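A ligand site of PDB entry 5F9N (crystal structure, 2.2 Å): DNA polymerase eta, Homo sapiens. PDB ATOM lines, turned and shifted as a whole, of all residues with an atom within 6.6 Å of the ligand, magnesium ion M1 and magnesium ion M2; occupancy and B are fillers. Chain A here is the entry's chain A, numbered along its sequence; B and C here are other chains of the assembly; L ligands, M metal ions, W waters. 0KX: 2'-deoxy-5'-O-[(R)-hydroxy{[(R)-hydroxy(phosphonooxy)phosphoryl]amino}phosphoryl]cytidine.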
ATOM      1  N   VAL A  15      15.050  -2.077  20.912  1.00  0.00           N
ATOM      2  CA  VAL A  15      16.238  -2.897  20.684  1.00  0.00           C
ATOM      3  C   VAL A  15      15.797  -4.320  20.390  1.00  0.00           C
ATOM      4  O   VAL A  15      14.946  -4.870  21.108  1.00  0.00           O
ATOM      5  CB  VAL A  15      17.192  -2.833  21.890  1.00  0.00           C
ATOM      6  CG1 VAL A  15      18.410  -3.690  21.634  1.00  0.00           C
ATOM      7  CG2 VAL A  15      17.592  -1.382  22.172  1.00  0.00           C
ATOM      8  N   ASP A  16      16.362  -4.921  19.352  1.00  0.00           N
ATOM      9  CA  ASP A  16      16.045  -6.285  18.971  1.00  0.00           C
ATOM     10  C   ASP A  16      17.315  -7.060  18.646  1.00  0.00           C
ATOM     11  O   ASP A  16      18.062  -6.680  17.745  1.00  0.00           O
ATOM     12  CB  ASP A  16      15.106  -6.305  17.766  1.00  0.00           C
ATOM     13  CG  ASP A  16      14.725  -7.689  17.384  1.00  0.00           C
ATOM     14  OD1 ASP A  16      13.610  -8.102  17.725  1.00  0.00           O
ATOM     15  OD2 ASP A  16      15.536  -8.386  16.761  1.00  0.00           O
ATOM     16  N   MET A  17      17.518  -8.175  19.355  1.00  0.00           N
ATOM     17  CA  MET A  17      18.709  -8.994  19.158  1.00  0.00           C
ATOM     18  C   MET A  17      18.713  -9.650  17.775  1.00  0.00           C
ATOM     19  O   MET A  17      17.712 -10.233  17.362  1.00  0.00           O
ATOM     20  CB  MET A  17      18.815 -10.077  20.245  1.00  0.00           C
ATOM     21  CG  MET A  17      18.578  -9.577  21.667  1.00  0.00           C
ATOM     22  SD  MET A  17      19.756  -8.297  22.169  1.00  0.00           S
ATOM     23  CE  MET A  17      21.308  -9.090  21.795  1.00  0.00           C
ATOM     24  N   ASP A  18      19.833  -9.551  17.082  1.00  0.00           N
ATOM     25  CA  ASP A  18      19.944 -10.179  15.765  1.00  0.00           C
ATOM     26  C   ASP A  18      19.966 -11.689  15.927  1.00  0.00           C
ATOM     27  O   ASP A  18      20.709 -12.211  16.770  1.00  0.00           O
ATOM     28  CB  ASP A  18      21.205  -9.698  15.066  1.00  0.00           C
ATOM     29  CG  ASP A  18      21.237  -8.192  14.869  1.00  0.00           C
ATOM     30  OD1 ASP A  18      20.172  -7.570  14.788  1.00  0.00           O
ATOM     31  OD2 ASP A  18      22.340  -7.622  14.786  1.00  0.00           O
ATOM     32  N   CYS A  19      19.154 -12.393  15.119  1.00  0.00           N
ATOM     33  CA  CYS A  19      18.950 -13.844  15.138  1.00  0.00           C
ATOM     34  C   CYS A  19      19.288 -14.452  16.504  1.00  0.00           C
ATOM     35  O   CYS A  19      20.274 -15.172  16.645  1.00  0.00           O
ATOM     36  CB  CYS A  19      19.765 -14.507  14.017  1.00  0.00           C
ATOM     37  SG  CYS A  19      21.554 -14.051  13.963  1.00  0.00           S
ATOM     38  N   PHE A  20      18.460 -14.151  17.503  1.00  0.00           N
ATOM     39  CA  PHE A  20      18.872 -14.240  18.903  1.00  0.00           C
ATOM     40  C   PHE A  20      19.230 -15.672  19.329  1.00  0.00           C
ATOM     41  O   PHE A  20      20.313 -15.912  19.880  1.00  0.00           O
ATOM     42  CB  PHE A  20      17.769 -13.675  19.781  1.00  0.00           C
ATOM     43  CG  PHE A  20      18.085 -13.684  21.222  1.00  0.00           C
ATOM     44  CD1 PHE A  20      19.316 -13.208  21.678  1.00  0.00           C
ATOM     45  CD2 PHE A  20      17.186 -14.179  22.138  1.00  0.00           C
ATOM     46  CE1 PHE A  20      19.639 -13.221  23.047  1.00  0.00           C
ATOM     47  CE2 PHE A  20      17.495 -14.205  23.510  1.00  0.00           C
ATOM     48  CZ  PHE A  20      18.718 -13.723  23.964  1.00  0.00           C
ATOM     49  N   PHE A  21      18.351 -16.647  19.055  1.00  0.00           N
ATOM     50  CA  PHE A  21      18.653 -18.021  19.470  1.00  0.00           C
ATOM     51  C   PHE A  21      19.948 -18.523  18.802  1.00  0.00           C
ATOM     52  O   PHE A  21      20.721 -19.264  19.406  1.00  0.00           O
ATOM     53  CB  PHE A  21      17.495 -18.968  19.150  1.00  0.00           C
ATOM     54  CG  PHE A  21      16.254 -18.775  20.011  1.00  0.00           C
ATOM     55  CD1 PHE A  21      16.060 -17.613  20.769  1.00  0.00           C
ATOM     56  CD2 PHE A  21      15.278 -19.758  20.053  1.00  0.00           C
ATOM     57  CE1 PHE A  21      14.900 -17.450  21.532  1.00  0.00           C
ATOM     58  CE2 PHE A  21      14.136 -19.610  20.843  1.00  0.00           C
ATOM     59  CZ  PHE A  21      13.952 -18.449  21.570  1.00  0.00           C
ATOM     60  N   VAL A  22      20.186 -18.120  17.551  1.00  0.00           N
ATOM     61  CA  VAL A  22      21.428 -18.496  16.854  1.00  0.00           C
ATOM     62  C   VAL A  22      22.647 -17.907  17.569  1.00  0.00           C
ATOM     63  O   VAL A  22      23.652 -18.604  17.800  1.00  0.00           O
ATOM     64  CB  VAL A  22      21.355 -18.058  15.385  1.00  0.00           C
ATOM     65  CG1 VAL A  22      22.699 -18.185  14.703  1.00  0.00           C
ATOM     66  CG2 VAL A  22      20.316 -18.878  14.626  1.00  0.00           C
ATOM     67  N   GLN A  41      14.161 -27.393  16.315  1.00  0.00           N
ATOM     68  CA  GLN A  41      13.583 -28.182  17.387  1.00  0.00           C
ATOM     69  C   GLN A  41      12.946 -29.439  16.809  1.00  0.00           C
ATOM     70  O   GLN A  41      12.321 -29.394  15.732  1.00  0.00           O
ATOM     71  CB  GLN A  41      12.579 -27.346  18.223  1.00  0.00           C
ATOM     72  CG  GLN A  41      11.384 -26.867  17.480  1.00  0.00           C
ATOM     73  CD  GLN A  41      10.492 -25.984  18.346  1.00  0.00           C
ATOM     74  OE1 GLN A  41      10.905 -25.521  19.398  1.00  0.00           O
ATOM     75  NE2 GLN A  41       9.255 -25.754  17.896  1.00  0.00           N
ATOM     76  N   ILE A  51      13.596 -22.388  13.825  1.00  0.00           N
ATOM     77  CA  ILE A  51      13.018 -21.236  14.515  1.00  0.00           C
ATOM     78  C   ILE A  51      13.931 -20.022  14.560  1.00  0.00           C
ATOM     79  O   ILE A  51      13.499 -18.969  15.063  1.00  0.00           O
ATOM     80  CB  ILE A  51      12.535 -21.581  15.944  1.00  0.00           C
ATOM     81  CG1 ILE A  51      13.701 -22.005  16.835  1.00  0.00           C
ATOM     82  CG2 ILE A  51      11.409 -22.634  15.916  1.00  0.00           C
ATOM     83  CD1 ILE A  51      13.275 -22.188  18.278  1.00  0.00           C
ATOM     84  N   ALA A  52      15.172 -20.120  14.111  1.00  0.00           N
ATOM     85  CA  ALA A  52      16.029 -18.945  14.005  1.00  0.00           C
ATOM     86  C   ALA A  52      17.103 -19.237  12.966  1.00  0.00           C
ATOM     87  O   ALA A  52      17.546 -20.377  12.821  1.00  0.00           O
ATOM     88  CB  ALA A  52      16.658 -18.563  15.361  1.00  0.00           C
ATOM     89  N   VAL A  53      17.492 -18.186  12.241  1.00  0.00           N
ATOM     90  CA  VAL A  53      18.356 -18.319  11.054  1.00  0.00           C
ATOM     91  C   VAL A  53      19.412 -17.235  11.077  1.00  0.00           C
ATOM     92  O   VAL A  53      19.071 -16.041  11.134  1.00  0.00           O
ATOM     93  CB  VAL A  53      17.556 -18.209   9.755  1.00  0.00           C
ATOM     94  CG1 VAL A  53      18.453 -18.556   8.567  1.00  0.00           C
ATOM     95  CG2 VAL A  53      16.326 -19.096   9.786  1.00  0.00           C
ATOM     96  N   TYR A  55      22.224 -14.672   9.525  1.00  0.00           N
ATOM     97  CA  TYR A  55      22.150 -13.883   8.303  1.00  0.00           C
ATOM     98  C   TYR A  55      22.946 -14.513   7.161  1.00  0.00           C
ATOM     99  O   TYR A  55      22.610 -14.305   5.997  1.00  0.00           O
ATOM    100  CB  TYR A  55      22.601 -12.444   8.573  1.00  0.00           C
ATOM    101  CG  TYR A  55      21.507 -11.653   9.255  1.00  0.00           C
ATOM    102  CD1 TYR A  55      21.282 -11.800  10.616  1.00  0.00           C
ATOM    103  CD2 TYR A  55      20.689 -10.777   8.548  1.00  0.00           C
ATOM    104  CE1 TYR A  55      20.277 -11.083  11.255  1.00  0.00           C
ATOM    105  CE2 TYR A  55      19.678 -10.069   9.178  1.00  0.00           C
ATOM    106  CZ  TYR A  55      19.467 -10.230  10.544  1.00  0.00           C
ATOM    107  OH  TYR A  55      18.464  -9.539  11.221  1.00  0.00           O
ATOM    108  N   ARG A  58      20.420 -16.896   5.840  1.00  0.00           N
ATOM    109  CA  ARG A  58      19.356 -16.148   5.163  1.00  0.00           C
ATOM    110  C   ARG A  58      19.706 -15.827   3.706  1.00  0.00           C
ATOM    111  O   ARG A  58      18.816 -15.814   2.851  1.00  0.00           O
ATOM    112  CB  ARG A  58      19.027 -14.854   5.923  1.00  0.00           C
ATOM    113  CG  ARG A  58      18.367 -15.077   7.290  1.00  0.00           C
ATOM    114  CD  ARG A  58      18.083 -13.760   8.038  1.00  0.00           C
ATOM    115  NE  ARG A  58      17.921 -14.007   9.474  1.00  0.00           N
ATOM    116  CZ  ARG A  58      17.395 -13.174  10.370  1.00  0.00           C
ATOM    117  NH1 ARG A  58      16.928 -11.968  10.015  1.00  0.00           N
ATOM    118  NH2 ARG A  58      17.319 -13.570  11.646  1.00  0.00           N
ATOM    119  N   ARG A  64      12.705 -19.042   8.867  1.00  0.00           N
ATOM    120  CA  ARG A  64      11.947 -19.599   9.982  1.00  0.00           C
ATOM    121  C   ARG A  64      10.802 -20.469   9.486  1.00  0.00           C
ATOM    122  O   ARG A  64      10.228 -20.225   8.424  1.00  0.00           O
ATOM    123  CB  ARG A  64      11.409 -18.435  10.829  1.00  0.00           C
ATOM    124  CG  ARG A  64      11.194 -18.710  12.287  1.00  0.00           C
ATOM    125  CD  ARG A  64      10.608 -17.475  12.985  1.00  0.00           C
ATOM    126  NE  ARG A  64       9.952 -16.560  12.034  1.00  0.00           N
ATOM    127  CZ  ARG A  64      10.413 -15.344  11.719  1.00  0.00           C
ATOM    128  NH1 ARG A  64      11.516 -14.875  12.299  1.00  0.00           N
ATOM    129  NH2 ARG A  64       9.769 -14.595  10.835  1.00  0.00           N
ATOM    130  N   LEU A  92      13.090 -23.873  26.600  1.00  0.00           N
ATOM    131  CA  LEU A  92      13.707 -22.628  26.148  1.00  0.00           C
ATOM    132  C   LEU A  92      14.540 -21.934  27.222  1.00  0.00           C
ATOM    133  O   LEU A  92      14.922 -20.775  27.040  1.00  0.00           O
ATOM    134  CB  LEU A  92      12.602 -21.693  25.614  1.00  0.00           C
ATOM    135  CG  LEU A  92      11.738 -22.313  24.506  1.00  0.00           C
ATOM    136  CD1 LEU A  92      10.741 -21.321  23.957  1.00  0.00           C
ATOM    137  CD2 LEU A  92      12.599 -22.864  23.370  1.00  0.00           C
ATOM    138  N   SER A 116       9.379  -9.040  24.177  1.00  0.00           N
ATOM    139  CA  SER A 116       9.470 -10.436  23.764  1.00  0.00           C
ATOM    140  C   SER A 116      10.725 -10.982  24.406  1.00  0.00           C
ATOM    141  O   SER A 116      11.416 -10.276  25.150  1.00  0.00           O
ATOM    142  CB  SER A 116       9.489 -10.582  22.233  1.00  0.00           C
ATOM    143  OG  SER A 116      10.753 -10.217  21.681  1.00  0.00           O
ATOM    144  N   ILE A 117      11.055 -12.233  24.103  1.00  0.00           N
ATOM    145  CA  ILE A 117      12.268 -12.803  24.674  1.00  0.00           C
ATOM    146  C   ILE A 117      13.521 -12.057  24.205  1.00  0.00           C
ATOM    147  O   ILE A 117      14.565 -12.100  24.886  1.00  0.00           O
ATOM    148  CB  ILE A 117      12.334 -14.307  24.350  1.00  0.00           C
ATOM    149  CG1 ILE A 117      13.312 -15.006  25.307  1.00  0.00           C
ATOM    150  CG2 ILE A 117      12.742 -14.537  22.893  1.00  0.00           C
ATOM    151  CD1 ILE A 117      13.147 -16.508  25.282  1.00  0.00           C
ATOM    152  N   ASP A 118      13.450 -11.345  23.077  1.00  0.00           N
ATOM    153  CA  ASP A 118      14.657 -10.702  22.569  1.00  0.00           C
ATOM    154  C   ASP A 118      14.458  -9.225  22.199  1.00  0.00           C
ATOM    155  O   ASP A 118      15.314  -8.663  21.499  1.00  0.00           O
ATOM    156  CB  ASP A 118      15.201 -11.468  21.375  1.00  0.00           C
ATOM    157  CG  ASP A 118      14.539 -11.089  20.090  1.00  0.00           C
ATOM    158  OD1 ASP A 118      13.292 -10.928  20.063  1.00  0.00           O
ATOM    159  OD2 ASP A 118      15.287 -10.918  19.089  1.00  0.00           O
ATOM    160  N   GLU A 119      13.381  -8.579  22.642  1.00  0.00           N
ATOM    161  CA  GLU A 119      13.145  -7.171  22.339  1.00  0.00           C
ATOM    162  C   GLU A 119      12.661  -6.435  23.568  1.00  0.00           C
ATOM    163  O   GLU A 119      11.874  -6.970  24.351  1.00  0.00           O
ATOM    164  CB  GLU A 119      12.081  -6.945  21.272  1.00  0.00           C
ATOM    165  CG  GLU A 119      12.153  -7.871  20.147  1.00  0.00           C
ATOM    166  CD  GLU A 119      11.036  -7.675  19.177  1.00  0.00           C
ATOM    167  OE1 GLU A 119      10.928  -8.516  18.290  1.00  0.00           O
ATOM    168  OE2 GLU A 119      10.268  -6.692  19.288  1.00  0.00           O
ATOM    169  N   SER A 216      20.155  -4.859  16.789  1.00  0.00           N
ATOM    170  CA  SER A 216      19.769  -3.666  16.071  1.00  0.00           C
ATOM    171  C   SER A 216      18.834  -2.823  16.943  1.00  0.00           C
ATOM    172  O   SER A 216      18.269  -3.317  17.915  1.00  0.00           O
ATOM    173  CB  SER A 216      19.079  -4.017  14.762  1.00  0.00           C
ATOM    174  OG  SER A 216      19.938  -4.794  13.958  1.00  0.00           O
ATOM    175  N   LYS A 234      18.870  -3.848   9.582  1.00  0.00           N
ATOM    176  CA  LYS A 234      19.409  -5.020  10.268  1.00  0.00           C
ATOM    177  C   LYS A 234      20.447  -5.722   9.389  1.00  0.00           C
ATOM    178  O   LYS A 234      20.341  -5.682   8.180  1.00  0.00           O
ATOM    179  CB  LYS A 234      18.297  -6.008  10.651  1.00  0.00           C
ATOM    180  CG  LYS A 234      17.632  -5.741  11.989  1.00  0.00           C
ATOM    181  CD  LYS A 234      16.588  -6.809  12.328  1.00  0.00           C
ATOM    182  CE  LYS A 234      16.180  -6.765  13.825  1.00  0.00           C
ATOM    183  NZ  LYS A 234      17.103  -7.556  14.760  1.00  0.00           N
ATOM    184  N   PRO A 235      21.441  -6.391   9.996  1.00  0.00           N
ATOM    185  CA  PRO A 235      21.743  -6.519  11.426  1.00  0.00           C
ATOM    186  C   PRO A 235      22.851  -5.574  11.949  1.00  0.00           C
ATOM    187  O   PRO A 235      23.468  -4.854  11.172  1.00  0.00           O
ATOM    188  CB  PRO A 235      22.206  -7.969  11.524  1.00  0.00           C
ATOM    189  CG  PRO A 235      22.961  -8.182  10.212  1.00  0.00           C
ATOM    190  CD  PRO A 235      22.177  -7.391   9.187  1.00  0.00           C
ATOM    191  P    DT B   8       6.599  -9.346  15.300  1.00  0.00           P
ATOM    192  OP1  DT B   8       7.443  -8.162  14.982  1.00  0.00           O
ATOM    193  OP2  DT B   8       6.196 -10.298  14.226  1.00  0.00           O
ATOM    194  O5'  DT B   8       7.358 -10.198  16.422  1.00  0.00           O
ATOM    195  C5'  DT B   8       7.647  -9.636  17.715  1.00  0.00           C
ATOM    196  C4'  DT B   8       8.450 -10.626  18.546  1.00  0.00           C
ATOM    197  O4'  DT B   8       7.603 -11.773  18.895  1.00  0.00           O
ATOM    198  C3'  DT B   8       9.663 -11.208  17.839  1.00  0.00           C
ATOM    199  O3'  DT B   8      10.736 -11.361  18.772  1.00  0.00           O
ATOM    200  C2'  DT B   8       9.149 -12.546  17.306  1.00  0.00           C
ATOM    201  C1'  DT B   8       8.175 -12.963  18.392  1.00  0.00           C
ATOM    202  N1   DT B   8       7.070 -13.859  17.918  1.00  0.00           N
ATOM    203  C2   DT B   8       6.820 -15.037  18.597  1.00  0.00           C
ATOM    204  O2   DT B   8       7.452 -15.388  19.570  1.00  0.00           O
ATOM    205  N3   DT B   8       5.791 -15.783  18.090  1.00  0.00           N
ATOM    206  C4   DT B   8       5.007 -15.492  17.004  1.00  0.00           C
ATOM    207  O4   DT B   8       4.091 -16.233  16.642  1.00  0.00           O
ATOM    208  C5   DT B   8       5.322 -14.251  16.324  1.00  0.00           C
ATOM    209  C7   DT B   8       4.531 -13.824  15.116  1.00  0.00           C
ATOM    210  C6   DT B   8       6.325 -13.496  16.805  1.00  0.00           C
ATOM    211  P    DT C   3       3.079 -27.438   8.366  1.00  0.00           P
ATOM    212  OP1  DT C   3       1.825 -27.406   7.583  1.00  0.00           O
ATOM    213  OP2  DT C   3       4.381 -27.083   7.727  1.00  0.00           O
ATOM    214  O5'  DT C   3       2.864 -26.484   9.626  1.00  0.00           O
ATOM    215  C5'  DT C   3       3.761 -25.414   9.876  1.00  0.00           C
ATOM    216  C4'  DT C   3       4.594 -25.721  11.097  1.00  0.00           C
ATOM    217  O4'  DT C   3       5.667 -24.742  11.222  1.00  0.00           O
ATOM    218  C3'  DT C   3       3.827 -25.684  12.434  1.00  0.00           C
ATOM    219  O3'  DT C   3       3.967 -26.957  13.117  1.00  0.00           O
ATOM    220  C2'  DT C   3       4.505 -24.546  13.205  1.00  0.00           C
ATOM    221  C1'  DT C   3       5.893 -24.561  12.592  1.00  0.00           C
ATOM    222  N1   DT C   3       6.659 -23.278  12.822  1.00  0.00           N
ATOM    223  C2   DT C   3       7.955 -23.339  13.336  1.00  0.00           C
ATOM    224  O2   DT C   3       8.540 -24.391  13.599  1.00  0.00           O
ATOM    225  N3   DT C   3       8.541 -22.105  13.519  1.00  0.00           N
ATOM    226  C4   DT C   3       7.973 -20.851  13.246  1.00  0.00           C
ATOM    227  O4   DT C   3       8.577 -19.799  13.438  1.00  0.00           O
ATOM    228  C5   DT C   3       6.628 -20.872  12.717  1.00  0.00           C
ATOM    229  C7   DT C   3       5.931 -19.591  12.391  1.00  0.00           C
ATOM    230  C6   DT C   3       6.042 -22.074  12.546  1.00  0.00           C
ATOM    231  P   GNE C   4       3.353 -27.199  14.588  1.00  0.00           P
ATOM    232  OP1 GNE C   4       3.457 -28.668  14.915  1.00  0.00           O
ATOM    233  OP2 GNE C   4       1.932 -26.696  14.691  1.00  0.00           O
ATOM    234  O5' GNE C   4       4.322 -26.383  15.591  1.00  0.00           O
ATOM    235  C5' GNE C   4       5.692 -26.752  15.707  1.00  0.00           C
ATOM    236  C4' GNE C   4       6.329 -26.131  16.947  1.00  0.00           C
ATOM    237  O4' GNE C   4       6.805 -24.803  16.698  1.00  0.00           O
ATOM    238  C3' GNE C   4       5.419 -26.034  18.160  1.00  0.00           C
ATOM    239  O3' GNE C   4       6.135 -26.791  19.106  1.00  0.00           O
ATOM    240  C2' GNE C   4       5.390 -24.561  18.538  1.00  0.00           C
ATOM    241  C1' GNE C   4       6.633 -23.997  17.878  1.00  0.00           C
ATOM    242  N9  GNE C   4       6.612 -22.578  17.428  1.00  0.00           N
ATOM    243  C8  GNE C   4       7.588 -21.657  17.653  1.00  0.00           C
ATOM    244  N7  GNE C   4       7.273 -20.474  17.070  1.00  0.00           N
ATOM    245  C5  GNE C   4       6.092 -20.629  16.449  1.00  0.00           C
ATOM    246  C6  GNE C   4       5.200 -19.775  15.646  1.00  0.00           C
ATOM    247  O6  GNE C   4       5.508 -18.588  15.418  1.00  0.00           O
ATOM    248  N1  GNE C   4       4.049 -20.295  15.169  1.00  0.00           N
ATOM    249  C2  GNE C   4       3.702 -21.586  15.411  1.00  0.00           C
ATOM    250  N2  GNE C   4       2.518 -21.823  14.812  1.00  0.00           N
ATOM    251  CM2 GNE C   4       2.107 -20.705  14.195  1.00  0.00           C
ATOM    252  N3  GNE C   4       4.495 -22.432  16.149  1.00  0.00           N
ATOM    253  C11 GNE C   4       3.068 -19.753  14.421  1.00  0.00           C
ATOM    254  C4  GNE C   4       5.668 -22.016  16.678  1.00  0.00           C
ATOM    255  P    DA C   5       5.570 -27.086  20.575  1.00  0.00           P
ATOM    256  OP1  DA C   5       6.338 -28.274  21.040  1.00  0.00           O
ATOM    257  OP2  DA C   5       4.083 -27.150  20.575  1.00  0.00           O
ATOM    258  O5'  DA C   5       6.051 -25.811  21.414  1.00  0.00           O
ATOM    259  C5'  DA C   5       7.445 -25.478  21.446  1.00  0.00           C
ATOM    260  C4'  DA C   5       7.665 -24.203  22.195  1.00  0.00           C
ATOM    261  O4'  DA C   5       7.283 -23.061  21.366  1.00  0.00           O
ATOM    262  C3'  DA C   5       6.861 -24.072  23.493  1.00  0.00           C
ATOM    263  O3'  DA C   5       7.672 -23.457  24.492  1.00  0.00           O
ATOM    264  C2'  DA C   5       5.694 -23.172  23.065  1.00  0.00           C
ATOM    265  C1'  DA C   5       6.385 -22.240  22.082  1.00  0.00           C
ATOM    266  N9   DA C   5       5.478 -21.634  21.116  1.00  0.00           N
ATOM    267  C8   DA C   5       4.346 -22.195  20.599  1.00  0.00           C
ATOM    268  N7   DA C   5       3.737 -21.423  19.723  1.00  0.00           N
ATOM    269  C5   DA C   5       4.517 -20.289  19.672  1.00  0.00           C
ATOM    270  C6   DA C   5       4.410 -19.089  18.940  1.00  0.00           C
ATOM    271  N6   DA C   5       3.422 -18.852  18.086  1.00  0.00           N
ATOM    272  N1   DA C   5       5.340 -18.154  19.125  1.00  0.00           N
ATOM    273  C2   DA C   5       6.341 -18.404  19.983  1.00  0.00           C
ATOM    274  N3   DA C   5       6.548 -19.489  20.726  1.00  0.00           N
ATOM    275  C4   DA C   5       5.591 -20.396  20.530  1.00  0.00           C
HETATM  276  PG  0KX L   1      16.129 -10.923  13.637  1.00  0.00           P
HETATM  277  O1G 0KX L   1      17.583 -10.510  13.456  1.00  0.00           O
HETATM  278  O2G 0KX L   1      15.337 -10.731  12.348  1.00  0.00           O
HETATM  279  O3G 0KX L   1      15.504 -10.180  14.787  1.00  0.00           O
HETATM  280  PB  0KX L   1      15.515 -13.124  15.286  1.00  0.00           P
HETATM  281  O1B 0KX L   1      15.929 -12.485  16.613  1.00  0.00           O
HETATM  282  O2B 0KX L   1      15.960 -14.581  15.218  1.00  0.00           O
HETATM  283  O3B 0KX L   1      16.102 -12.454  13.988  1.00  0.00           O
HETATM  284  PA  0KX L   1      12.822 -12.459  16.213  1.00  0.00           P
HETATM  285  O1A 0KX L   1      11.515 -12.241  15.489  1.00  0.00           O
HETATM  286  O2A 0KX L   1      13.350 -11.151  16.746  1.00  0.00           O
HETATM  287  N3A 0KX L   1      13.864 -13.100  15.099  1.00  0.00           N
HETATM  288  O5' 0KX L   1      12.626 -13.510  17.405  1.00  0.00           O
HETATM  289  C5' 0KX L   1      13.643 -13.729  18.382  1.00  0.00           C
HETATM  290  C4' 0KX L   1      13.692 -15.070  18.772  1.00  0.00           C
HETATM  291  O4' 0KX L   1      12.260 -15.624  19.140  1.00  0.00           O
HETATM  292  C3' 0KX L   1      14.168 -15.965  17.606  1.00  0.00           C
HETATM  293  O3' 0KX L   1      15.653 -16.091  17.606  1.00  0.00           O
HETATM  294  C2' 0KX L   1      13.541 -17.119  17.824  1.00  0.00           C
HETATM  295  C1' 0KX L   1      12.177 -16.829  18.646  1.00  0.00           C
HETATM  296  N1  0KX L   1      11.005 -16.892  17.824  1.00  0.00           N
HETATM  297  C2  0KX L   1      10.137 -18.089  17.820  1.00  0.00           C
HETATM  298  N3  0KX L   1       8.948 -18.122  16.968  1.00  0.00           N
HETATM  299  C4  0KX L   1       8.630 -17.023  16.126  1.00  0.00           C
HETATM  300  C5  0KX L   1       9.492 -15.822  16.118  1.00  0.00           C
HETATM  301  C6  0KX L   1      10.681 -15.786  16.980  1.00  0.00           C
HETATM  302  O2  0KX L   1      10.400 -19.047  18.524  1.00  0.00           O
HETATM  303  N4  0KX L   1       7.481 -17.038  15.294  1.00  0.00           N
HETATM  304 MG    MG M   1      15.426 -10.414  16.967  1.00  0.00          MG
HETATM  305 MG    MG M   2      12.404  -9.833  18.300  1.00  0.00          MG
HETATM  306  O   HOH W   1      11.558  -9.237  16.291  1.00  0.00           O
HETATM  307  O   HOH W   2       9.884 -16.478  20.793  1.00  0.00           O
HETATM  308  O   HOH W   3      13.282  -8.979  14.285  1.00  0.00           O
HETATM  309  O   HOH W   4       7.449 -14.727  13.579  1.00  0.00           O
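Water W4 lies within hydrogen-bond range of N4 of the ligand (2.9 Å) and NE of Arg 64 (3.5 Å).
Water W2 lies within hydrogen-bond range of O2 of DT 8 of chain B (2.9 Å) and an oxygen (O4') of the ligand (3.0 Å).
Magnesium ion M2 is bound by OE1 of Glu 119, OD1 of Asp 16, O2A of the ligand, OD1 of Asp 118, water W1 and O3' of DT 8 of chain B.
Magnesium ion M2 has six donor atoms within binding distance.
Residues that only touch magnesium ion M2: Ser 116.
Within 4 Å of magnesium ion M2: Asp 16, Ser 116, Asp 118, Glu 119 and DT 8 of chain B.
O of Asp 16 sits at hydrogen-bond distance from NZ of Lys 234 (3.3 Å).
NH1 of Arg 58 lies within hydrogen-bond range of OH of Tyr 55.
N of Asp 118 lies close to OG of Ser 116, at 3.2 Å.
The side-chain hydroxyl (OG) of Ser 116 lies close to O3' of DT 8 of chain B.
The side-chain hydroxyl (OG) of Ser 216 lies within hydrogen-bond range of the side-chain carboxylate (OD1) of Asp 18 (2.9 Å).
N of Asp 16 is in hydrogen-bond range of O of Ser 216 (2.9 Å).
N1 of DA 5 of chain C lies close to N3 of DT 8 of chain B, at 2.6 Å.
The side-chain amide nitrogen of Gln 41 lies within hydrogen-bond range of O4' of GNE 4 of chain C (2.9 Å).
CA of Asp 18 touches O1G of the ligand, at 3.3 Å.
Ile 51 touches the ligand.
Ala 52 touches the ligand.
Arg 64 touches the ligand (CD to C5, 3.7 Å).
CG2 of Ile 117 touches O4' of the ligand, at 3.9 Å.
DT 3 of chain C touches the ligand.
DA 5 of chain C touches the ligand (C2 to N3, 3.996 Å).
Hydrophobic or aromatic side chains within 4 Å of the ligand: Phe 20, Phe 21, Ala 52, Tyr 55 and Ile 117.
Within 4 Å of the ligand: Asp 16, Met 17, Asp 18, Cys 19, Phe 20, Phe 21, Ile 51, Ala 52, Tyr 55, Arg 58, Arg 64, Ile 117, Asp 118, Glu 119, Lys 234, DT 8 of chain B, DT 3 of chain C, GNE 4 of chain C and DA 5 of chain C.
Lys 234 touches magnesium ion M1 (NZ to MG, 3.98 Å).
Of the 27 residues printed, 4 come within 4 Å of magnesium ion M1.
The nearest printed residue that does not touch magnesium ion M1 is Asp 18 (4.5 Å).
Magnesium ion M1 is bound by OD2 of Asp 16 (2.0 Å), O1B of the ligand (2.2 Å), OD2 of Asp 118 (2.2 Å), O3G of the ligand (2.2 Å), O2A of the ligand (2.2 Å) and O of Met 17 (2.3 Å).
N of Cys 19 lies within hydrogen-bond range of O1G of the ligand, at 3.0 Å.
The backbone NH (N) of Phe 21 is in hydrogen-bond range of an oxygen (O3') of the ligand, at 3.1 Å.
An oxygen (O1G) of the ligand is in salt-bridge range of the side-chain amino group (NZ) of Lys 234.
O6 of GNE 4 of chain C is in hydrogen-bond range of N4 of the ligand, at 2.5 Å.
The side-chain hydroxyl (OH) of Tyr 55 sits at hydrogen-bond distance from an oxygen (O1G) of the ligand.
The guanidinium group (NH1) of Arg 58 is in salt-bridge range of an oxygen (O2G) of the ligand.
An oxygen (O3') of the ligand lies within hydrogen-bond range of the backbone NH (N) of Phe 20, 3.4 Å away.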
